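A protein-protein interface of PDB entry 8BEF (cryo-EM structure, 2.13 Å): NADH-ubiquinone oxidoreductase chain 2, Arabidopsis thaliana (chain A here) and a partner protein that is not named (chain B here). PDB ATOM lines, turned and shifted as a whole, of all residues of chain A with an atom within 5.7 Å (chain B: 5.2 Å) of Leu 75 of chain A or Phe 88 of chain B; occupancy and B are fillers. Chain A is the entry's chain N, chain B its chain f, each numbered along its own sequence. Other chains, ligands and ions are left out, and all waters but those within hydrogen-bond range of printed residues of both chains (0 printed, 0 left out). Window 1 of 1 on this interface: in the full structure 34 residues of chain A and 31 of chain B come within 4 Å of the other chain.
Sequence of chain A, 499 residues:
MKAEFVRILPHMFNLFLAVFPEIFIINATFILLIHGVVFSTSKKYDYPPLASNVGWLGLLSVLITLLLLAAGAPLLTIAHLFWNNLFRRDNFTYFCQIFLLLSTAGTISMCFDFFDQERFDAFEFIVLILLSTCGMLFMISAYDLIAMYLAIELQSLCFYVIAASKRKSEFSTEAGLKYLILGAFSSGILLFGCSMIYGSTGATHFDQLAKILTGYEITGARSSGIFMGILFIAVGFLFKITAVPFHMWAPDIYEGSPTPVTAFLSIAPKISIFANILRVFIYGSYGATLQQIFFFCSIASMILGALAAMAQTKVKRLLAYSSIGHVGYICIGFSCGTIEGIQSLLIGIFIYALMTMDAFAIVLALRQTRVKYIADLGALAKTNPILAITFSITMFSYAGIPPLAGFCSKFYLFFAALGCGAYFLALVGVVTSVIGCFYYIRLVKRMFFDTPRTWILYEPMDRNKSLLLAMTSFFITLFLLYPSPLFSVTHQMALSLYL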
ATOM      1  N   LEU A  17      -1.918  14.364  17.954  1.00  0.00           N
ATOM      2  CA  LEU A  17      -1.542  13.456  16.879  1.00  0.00           C
ATOM      3  C   LEU A  17      -0.263  13.915  16.192  1.00  0.00           C
ATOM      4  O   LEU A  17       0.485  13.090  15.661  1.00  0.00           O
ATOM      5  CB  LEU A  17      -2.678  13.338  15.862  1.00  0.00           C
ATOM      6  CG  LEU A  17      -3.870  12.482  16.293  1.00  0.00           C
ATOM      7  CD1 LEU A  17      -5.023  12.628  15.309  1.00  0.00           C
ATOM      8  CD2 LEU A  17      -3.452  11.028  16.436  1.00  0.00           C
ATOM      9  N   ALA A  18       0.011  15.223  16.210  1.00  0.00           N
ATOM     10  CA  ALA A  18       1.247  15.745  15.640  1.00  0.00           C
ATOM     11  C   ALA A  18       2.487  15.272  16.391  1.00  0.00           C
ATOM     12  O   ALA A  18       3.595  15.381  15.856  1.00  0.00           O
ATOM     13  CB  ALA A  18       1.213  17.276  15.622  1.00  0.00           C
ATOM     14  N   GLY A  72       1.730   7.706   9.597  1.00  0.00           N
ATOM     15  CA  GLY A  72       0.897   8.859   9.874  1.00  0.00           C
ATOM     16  C   GLY A  72       1.417  10.144   9.265  1.00  0.00           C
ATOM     17  O   GLY A  72       1.410  11.189   9.921  1.00  0.00           O
ATOM     18  N   ALA A  73       1.875  10.079   8.013  1.00  0.00           N
ATOM     19  CA  ALA A  73       2.521  11.235   7.396  1.00  0.00           C
ATOM     20  C   ALA A  73       1.645  12.484   7.389  1.00  0.00           C
ATOM     21  O   ALA A  73       2.106  13.530   7.879  1.00  0.00           O
ATOM     22  CB  ALA A  73       2.991  10.865   5.984  1.00  0.00           C
ATOM     23  N   PRO A  74       0.400  12.465   6.888  1.00  0.00           N
ATOM     24  CA  PRO A  74      -0.424  13.686   6.993  1.00  0.00           C
ATOM     25  C   PRO A  74      -0.705  14.115   8.424  1.00  0.00           C
ATOM     26  O   PRO A  74      -0.749  15.318   8.706  1.00  0.00           O
ATOM     27  CB  PRO A  74      -1.721  13.321   6.256  1.00  0.00           C
ATOM     28  CG  PRO A  74      -1.503  12.004   5.630  1.00  0.00           C
ATOM     29  CD  PRO A  74      -0.337  11.348   6.273  1.00  0.00           C
ATOM     30  N   LEU A  75      -0.892  13.165   9.340  1.00  0.00           N
ATOM     31  CA  LEU A  75      -1.312  13.520  10.693  1.00  0.00           C
ATOM     32  C   LEU A  75      -0.244  14.313  11.436  1.00  0.00           C
ATOM     33  O   LEU A  75      -0.572  15.078  12.349  1.00  0.00           O
ATOM     34  CB  LEU A  75      -1.683  12.265  11.477  1.00  0.00           C
ATOM     35  CG  LEU A  75      -2.817  11.433  10.878  1.00  0.00           C
ATOM     36  CD1 LEU A  75      -3.029  10.171  11.684  1.00  0.00           C
ATOM     37  CD2 LEU A  75      -4.096  12.242  10.801  1.00  0.00           C
ATOM     38  N   LEU A  76       1.027  14.153  11.061  1.00  0.00           N
ATOM     39  CA  LEU A  76       2.094  14.907  11.707  1.00  0.00           C
ATOM     40  C   LEU A  76       1.976  16.406  11.457  1.00  0.00           C
ATOM     41  O   LEU A  76       2.577  17.193  12.193  1.00  0.00           O
ATOM     42  CB  LEU A  76       3.456  14.398  11.231  1.00  0.00           C
ATOM     43  CG  LEU A  76       3.744  12.913  11.464  1.00  0.00           C
ATOM     44  CD1 LEU A  76       4.986  12.478  10.703  1.00  0.00           C
ATOM     45  CD2 LEU A  76       3.896  12.625  12.950  1.00  0.00           C
ATOM     46  N   THR A  77       1.222  16.815  10.439  1.00  0.00           N
ATOM     47  CA  THR A  77       0.992  18.223  10.141  1.00  0.00           C
ATOM     48  C   THR A  77      -0.315  18.748  10.717  1.00  0.00           C
ATOM     49  O   THR A  77      -0.673  19.899  10.456  1.00  0.00           O
ATOM     50  CB  THR A  77       1.002  18.450   8.630  1.00  0.00           C
ATOM     51  OG1 THR A  77       0.010  17.618   8.023  1.00  0.00           O
ATOM     52  CG2 THR A  77       2.366  18.110   8.053  1.00  0.00           C
ATOM     53  N   ILE A  78      -1.047  17.930  11.472  1.00  0.00           N
ATOM     54  CA  ILE A  78      -2.301  18.382  12.055  1.00  0.00           C
ATOM     55  C   ILE A  78      -2.028  19.487  13.071  1.00  0.00           C
ATOM     56  O   ILE A  78      -0.970  19.530  13.714  1.00  0.00           O
ATOM     57  CB  ILE A  78      -3.058  17.203  12.693  1.00  0.00           C
ATOM     58  CG1 ILE A  78      -4.562  17.341  12.462  1.00  0.00           C
ATOM     59  CG2 ILE A  78      -2.773  17.099  14.189  1.00  0.00           C
ATOM     60  CD1 ILE A  78      -5.380  16.284  13.175  1.00  0.00           C
ATOM     61  N   ALA B   7      -5.026  21.365   9.649  1.00  0.00           N
ATOM     62  CA  ALA B   7      -3.761  20.806   9.205  1.00  0.00           C
ATOM     63  C   ALA B   7      -3.190  21.616   8.048  1.00  0.00           C
ATOM     64  O   ALA B   7      -3.893  22.371   7.376  1.00  0.00           O
ATOM     65  CB  ALA B   7      -3.930  19.345   8.786  1.00  0.00           C
ATOM     66  N   GLU B   9      -1.673  20.211   5.274  1.00  0.00           N
ATOM     67  CA  GLU B   9      -2.102  19.521   4.063  1.00  0.00           C
ATOM     68  C   GLU B   9      -3.532  19.033   4.248  1.00  0.00           C
ATOM     69  O   GLU B   9      -3.808  18.229   5.144  1.00  0.00           O
ATOM     70  CB  GLU B   9      -1.170  18.355   3.734  1.00  0.00           C
ATOM     71  CG  GLU B   9      -0.534  17.701   4.936  1.00  0.00           C
ATOM     72  CD  GLU B   9       0.484  16.643   4.551  1.00  0.00           C
ATOM     73  OE1 GLU B   9       0.234  15.901   3.579  1.00  0.00           O
ATOM     74  OE2 GLU B   9       1.533  16.554   5.222  1.00  0.00           O
ATOM     75  N   LYS B  10      -4.429  19.512   3.393  1.00  0.00           N
ATOM     76  CA  LYS B  10      -5.851  19.241   3.530  1.00  0.00           C
ATOM     77  C   LYS B  10      -6.154  17.759   3.319  1.00  0.00           C
ATOM     78  O   LYS B  10      -5.406  17.026   2.668  1.00  0.00           O
ATOM     79  CB  LYS B  10      -6.651  20.082   2.535  1.00  0.00           C
ATOM     80  CG  LYS B  10      -7.282  21.331   3.133  1.00  0.00           C
ATOM     81  CD  LYS B  10      -6.261  22.181   3.869  1.00  0.00           C
ATOM     82  CE  LYS B  10      -6.927  23.345   4.584  1.00  0.00           C
ATOM     83  NZ  LYS B  10      -5.996  24.019   5.531  1.00  0.00           N
ATOM     84  N   ALA B  11      -7.273  17.326   3.896  1.00  0.00           N
ATOM     85  CA  ALA B  11      -7.736  15.954   3.735  1.00  0.00           C
ATOM     86  C   ALA B  11      -8.168  15.691   2.296  1.00  0.00           C
ATOM     87  O   ALA B  11      -8.842  16.514   1.673  1.00  0.00           O
ATOM     88  CB  ALA B  11      -8.898  15.676   4.688  1.00  0.00           C
ATOM     89  N   GLN B  12      -7.783  14.527   1.774  1.00  0.00           N
ATOM     90  CA  GLN B  12      -8.105  14.132   0.409  1.00  0.00           C
ATOM     91  C   GLN B  12      -9.333  13.234   0.324  1.00  0.00           C
ATOM     92  O   GLN B  12      -9.639  12.723  -0.757  1.00  0.00           O
ATOM     93  CB  GLN B  12      -6.908  13.432  -0.233  1.00  0.00           C
ATOM     94  CG  GLN B  12      -5.608  14.199  -0.121  1.00  0.00           C
ATOM     95  CD  GLN B  12      -4.414  13.371  -0.544  1.00  0.00           C
ATOM     96  OE1 GLN B  12      -4.347  12.173  -0.270  1.00  0.00           O
ATOM     97  NE2 GLN B  12      -3.462  14.006  -1.218  1.00  0.00           N
ATOM     98  N   TYR B  13     -10.035  13.028   1.426  1.00  0.00           N
ATOM     99  CA  TYR B  13     -11.216  12.183   1.488  1.00  0.00           C
ATOM    100  C   TYR B  13     -12.300  12.914   2.262  1.00  0.00           C
ATOM    101  O   TYR B  13     -12.006  13.846   3.017  1.00  0.00           O
ATOM    102  CB  TYR B  13     -10.885  10.834   2.148  1.00  0.00           C
ATOM    103  CG  TYR B  13      -9.755  10.110   1.461  1.00  0.00           C
ATOM    104  CD1 TYR B  13      -9.967   9.401   0.282  1.00  0.00           C
ATOM    105  CD2 TYR B  13      -8.468  10.151   1.977  1.00  0.00           C
ATOM    106  CE1 TYR B  13      -8.927   8.747  -0.353  1.00  0.00           C
ATOM    107  CE2 TYR B  13      -7.427   9.503   1.352  1.00  0.00           C
ATOM    108  CZ  TYR B  13      -7.660   8.803   0.188  1.00  0.00           C
ATOM    109  OH  TYR B  13      -6.618   8.158  -0.433  1.00  0.00           O
ATOM    110  N   GLN B  79      -4.602   6.341  15.670  1.00  0.00           N
ATOM    111  CA  GLN B  79      -4.121   7.114  14.534  1.00  0.00           C
ATOM    112  C   GLN B  79      -4.928   6.795  13.287  1.00  0.00           C
ATOM    113  O   GLN B  79      -5.442   7.696  12.615  1.00  0.00           O
ATOM    114  CB  GLN B  79      -2.643   6.796  14.306  1.00  0.00           C
ATOM    115  CG  GLN B  79      -1.746   7.974  14.095  1.00  0.00           C
ATOM    116  CD  GLN B  79      -0.287   7.571  14.098  1.00  0.00           C
ATOM    117  OE1 GLN B  79       0.437   7.832  15.057  1.00  0.00           O
ATOM    118  NE2 GLN B  79       0.150   6.920  13.028  1.00  0.00           N
ATOM    119  N   GLY B  83      -7.638   9.336  11.643  1.00  0.00           N
ATOM    120  CA  GLY B  83      -7.334   9.780  10.298  1.00  0.00           C
ATOM    121  C   GLY B  83      -8.429   9.446   9.306  1.00  0.00           C
ATOM    122  O   GLY B  83      -8.688  10.222   8.383  1.00  0.00           O
ATOM    123  N   ARG B  84      -9.087   8.298   9.483  1.00  0.00           N
ATOM    124  CA  ARG B  84     -10.210   7.951   8.617  1.00  0.00           C
ATOM    125  C   ARG B  84     -11.389   8.887   8.850  1.00  0.00           C
ATOM    126  O   ARG B  84     -11.985   9.396   7.896  1.00  0.00           O
ATOM    127  CB  ARG B  84     -10.623   6.492   8.835  1.00  0.00           C
ATOM    128  CG  ARG B  84      -9.663   5.479   8.226  1.00  0.00           C
ATOM    129  CD  ARG B  84     -10.317   4.116   8.030  1.00  0.00           C
ATOM    130  NE  ARG B  84     -10.945   3.610   9.245  1.00  0.00           N
ATOM    131  CZ  ARG B  84     -10.299   3.011  10.236  1.00  0.00           C
ATOM    132  NH1 ARG B  84      -8.990   2.829  10.199  1.00  0.00           N
ATOM    133  NH2 ARG B  84     -10.986   2.582  11.291  1.00  0.00           N
ATOM    134  N   MET B  86     -11.316  11.875   9.928  1.00  0.00           N
ATOM    135  CA  MET B  86     -10.945  13.225   9.519  1.00  0.00           C
ATOM    136  C   MET B  86     -10.745  13.368   8.016  1.00  0.00           C
ATOM    137  O   MET B  86     -10.567  14.492   7.538  1.00  0.00           O
ATOM    138  CB  MET B  86      -9.666  13.654  10.245  1.00  0.00           C
ATOM    139  CG  MET B  86      -9.801  13.784  11.756  1.00  0.00           C
ATOM    140  SD  MET B  86      -8.230  14.265  12.506  1.00  0.00           S
ATOM    141  CE  MET B  86      -8.767  14.956  14.062  1.00  0.00           C
ATOM    142  N   GLY B  87     -10.770  12.271   7.266  1.00  0.00           N
ATOM    143  CA  GLY B  87     -10.586  12.324   5.834  1.00  0.00           C
ATOM    144  C   GLY B  87      -9.153  12.292   5.356  1.00  0.00           C
ATOM    145  O   GLY B  87      -8.916  12.498   4.162  1.00  0.00           O
ATOM    146  N   PHE B  88      -8.191  12.042   6.246  1.00  0.00           N
ATOM    147  CA  PHE B  88      -6.795  11.956   5.835  1.00  0.00           C
ATOM    148  C   PHE B  88      -6.440  10.588   5.263  1.00  0.00           C
ATOM    149  O   PHE B  88      -5.494  10.482   4.477  1.00  0.00           O
ATOM    150  CB  PHE B  88      -5.877  12.286   7.013  1.00  0.00           C
ATOM    151  CG  PHE B  88      -5.953  13.717   7.456  1.00  0.00           C
ATOM    152  CD1 PHE B  88      -5.437  14.728   6.665  1.00  0.00           C
ATOM    153  CD2 PHE B  88      -6.544  14.053   8.662  1.00  0.00           C
ATOM    154  CE1 PHE B  88      -5.506  16.049   7.068  1.00  0.00           C
ATOM    155  CE2 PHE B  88      -6.617  15.375   9.072  1.00  0.00           C
ATOM    156  CZ  PHE B  88      -6.097  16.372   8.272  1.00  0.00           C
ATOM    157  N   PHE B  89      -7.164   9.544   5.642  1.00  0.00           N
ATOM    158  CA  PHE B  89      -6.960   8.198   5.135  1.00  0.00           C
ATOM    159  C   PHE B  89      -8.205   7.729   4.397  1.00  0.00           C
ATOM    160  O   PHE B  89      -9.308   8.227   4.650  1.00  0.00           O
ATOM    161  CB  PHE B  89      -6.637   7.208   6.266  1.00  0.00           C
ATOM    162  CG  PHE B  89      -5.426   7.568   7.076  1.00  0.00           C
ATOM    163  CD1 PHE B  89      -4.270   8.017   6.464  1.00  0.00           C
ATOM    164  CD2 PHE B  89      -5.436   7.427   8.456  1.00  0.00           C
ATOM    165  CE1 PHE B  89      -3.153   8.338   7.212  1.00  0.00           C
ATOM    166  CE2 PHE B  89      -4.321   7.744   9.209  1.00  0.00           C
ATOM    167  CZ  PHE B  89      -3.179   8.202   8.587  1.00  0.00           C
ATOM    168  N   PRO B  90      -8.063   6.782   3.467  1.00  0.00           N
ATOM    169  CA  PRO B  90      -9.242   6.205   2.806  1.00  0.00           C
ATOM    170  C   PRO B  90     -10.264   5.709   3.820  1.00  0.00           C
ATOM    171  O   PRO B  90      -9.949   4.909   4.704  1.00  0.00           O
ATOM    172  CB  PRO B  90      -8.640   5.053   1.996  1.00  0.00           C
ATOM    173  CG  PRO B  90      -7.312   5.587   1.606  1.00  0.00           C
ATOM    174  CD  PRO B  90      -6.820   6.241   2.889  1.00  0.00           C
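The backbone carbonyl oxygen (O) of Ala 7 of chain B is in hydrogen-bond range of the side-chain amino group (NZ) of Lys 10 of chain B.
N of Phe 88 of chain B is in hydrogen-bond range of O of Gly 83 of chain B, at 2.9 Å.
The backbone NH (N) of Phe 89 of chain B is in hydrogen-bond range of the backbone carbonyl oxygen (O) of Gly 83 of chain B (3.2 Å).
OG1 of Thr 77 of chain A sits at hydrogen-bond distance from O of Pro 74 of chain A (2.5 Å).
Leu 75 of chain A touches just these residues of chain B: Gln 79 (3.5 Å), Phe 88 (3.7 Å) and Phe 89 (3.7 Å).
Of the printed residues of chain B, Ile 78 of chain A touches Ala 7 and Met 86.
Printed residues of chain A within 4 Å of Ala 7 of chain B: Thr 77 (3.5 Å) and Ile 78 (3.8 Å).
Printed residues of chain A within 4 Å of Glu 9 of chain B: Pro 74 and Thr 77.
Lys 10 of chain B touches none of the printed residues of chain A.
Gly 87 of chain B touches none of the printed residues of chain A.
Of the printed residues of chain A, Phe 88 of chain B touches Pro 74 (3.99 Å) and Leu 75 (3.7 Å).
The nearest residue of chain B that does not touch Leu 75 of chain A is Gly 83 of chain B (4.1 Å).
The nearest printed residue of chain A that does not touch Phe 88 of chain B is Ile 78 of chain A (4.4 Å).
Gly 72 of chain A touches Gln 79 of chain B (CA to NE2, 3.8 Å).
Glu 9 of chain B touches Pro 74 of chain A.
Phe 88 of chain B touches Pro 74 of chain A (CD1 to CB, 3.99 Å).
CD1 of Leu 75 of chain A touches CG of Gln 79 of chain B (3.5 Å).
CD2 of Leu 75 of chain A touches CD2 of Phe 88 of chain B, at 3.7 Å.
CZ of Phe 89 of chain B touches CD1 of Leu 75 of chain A, at 3.7 Å.
Thr 77 of chain A touches Ala 7 of chain B.
Ile 78 of chain A touches Ala 7 of chain B (CA to CB, 3.8 Å).
Met 86 of chain B touches Ile 78 of chain A.
The side-chain hydroxyl of Thr 77 of chain A lies close to the side-chain carboxylate of Glu 9 of chain B.
Printed residues of chain A that touch a printed residue of chain B: Gly 72, Pro 74, Leu 75, Thr 77 and Ile 78.
Hydrophobic or aromatic side chains of chain B that line the printed part of chain A: Ala 7, Met 86, Phe 88 and Phe 89.
Along chain B the printed residues that touch a printed residue of chain A span positions 7 to 89.
Among the printed residues, 10 pairs touch across the chains.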
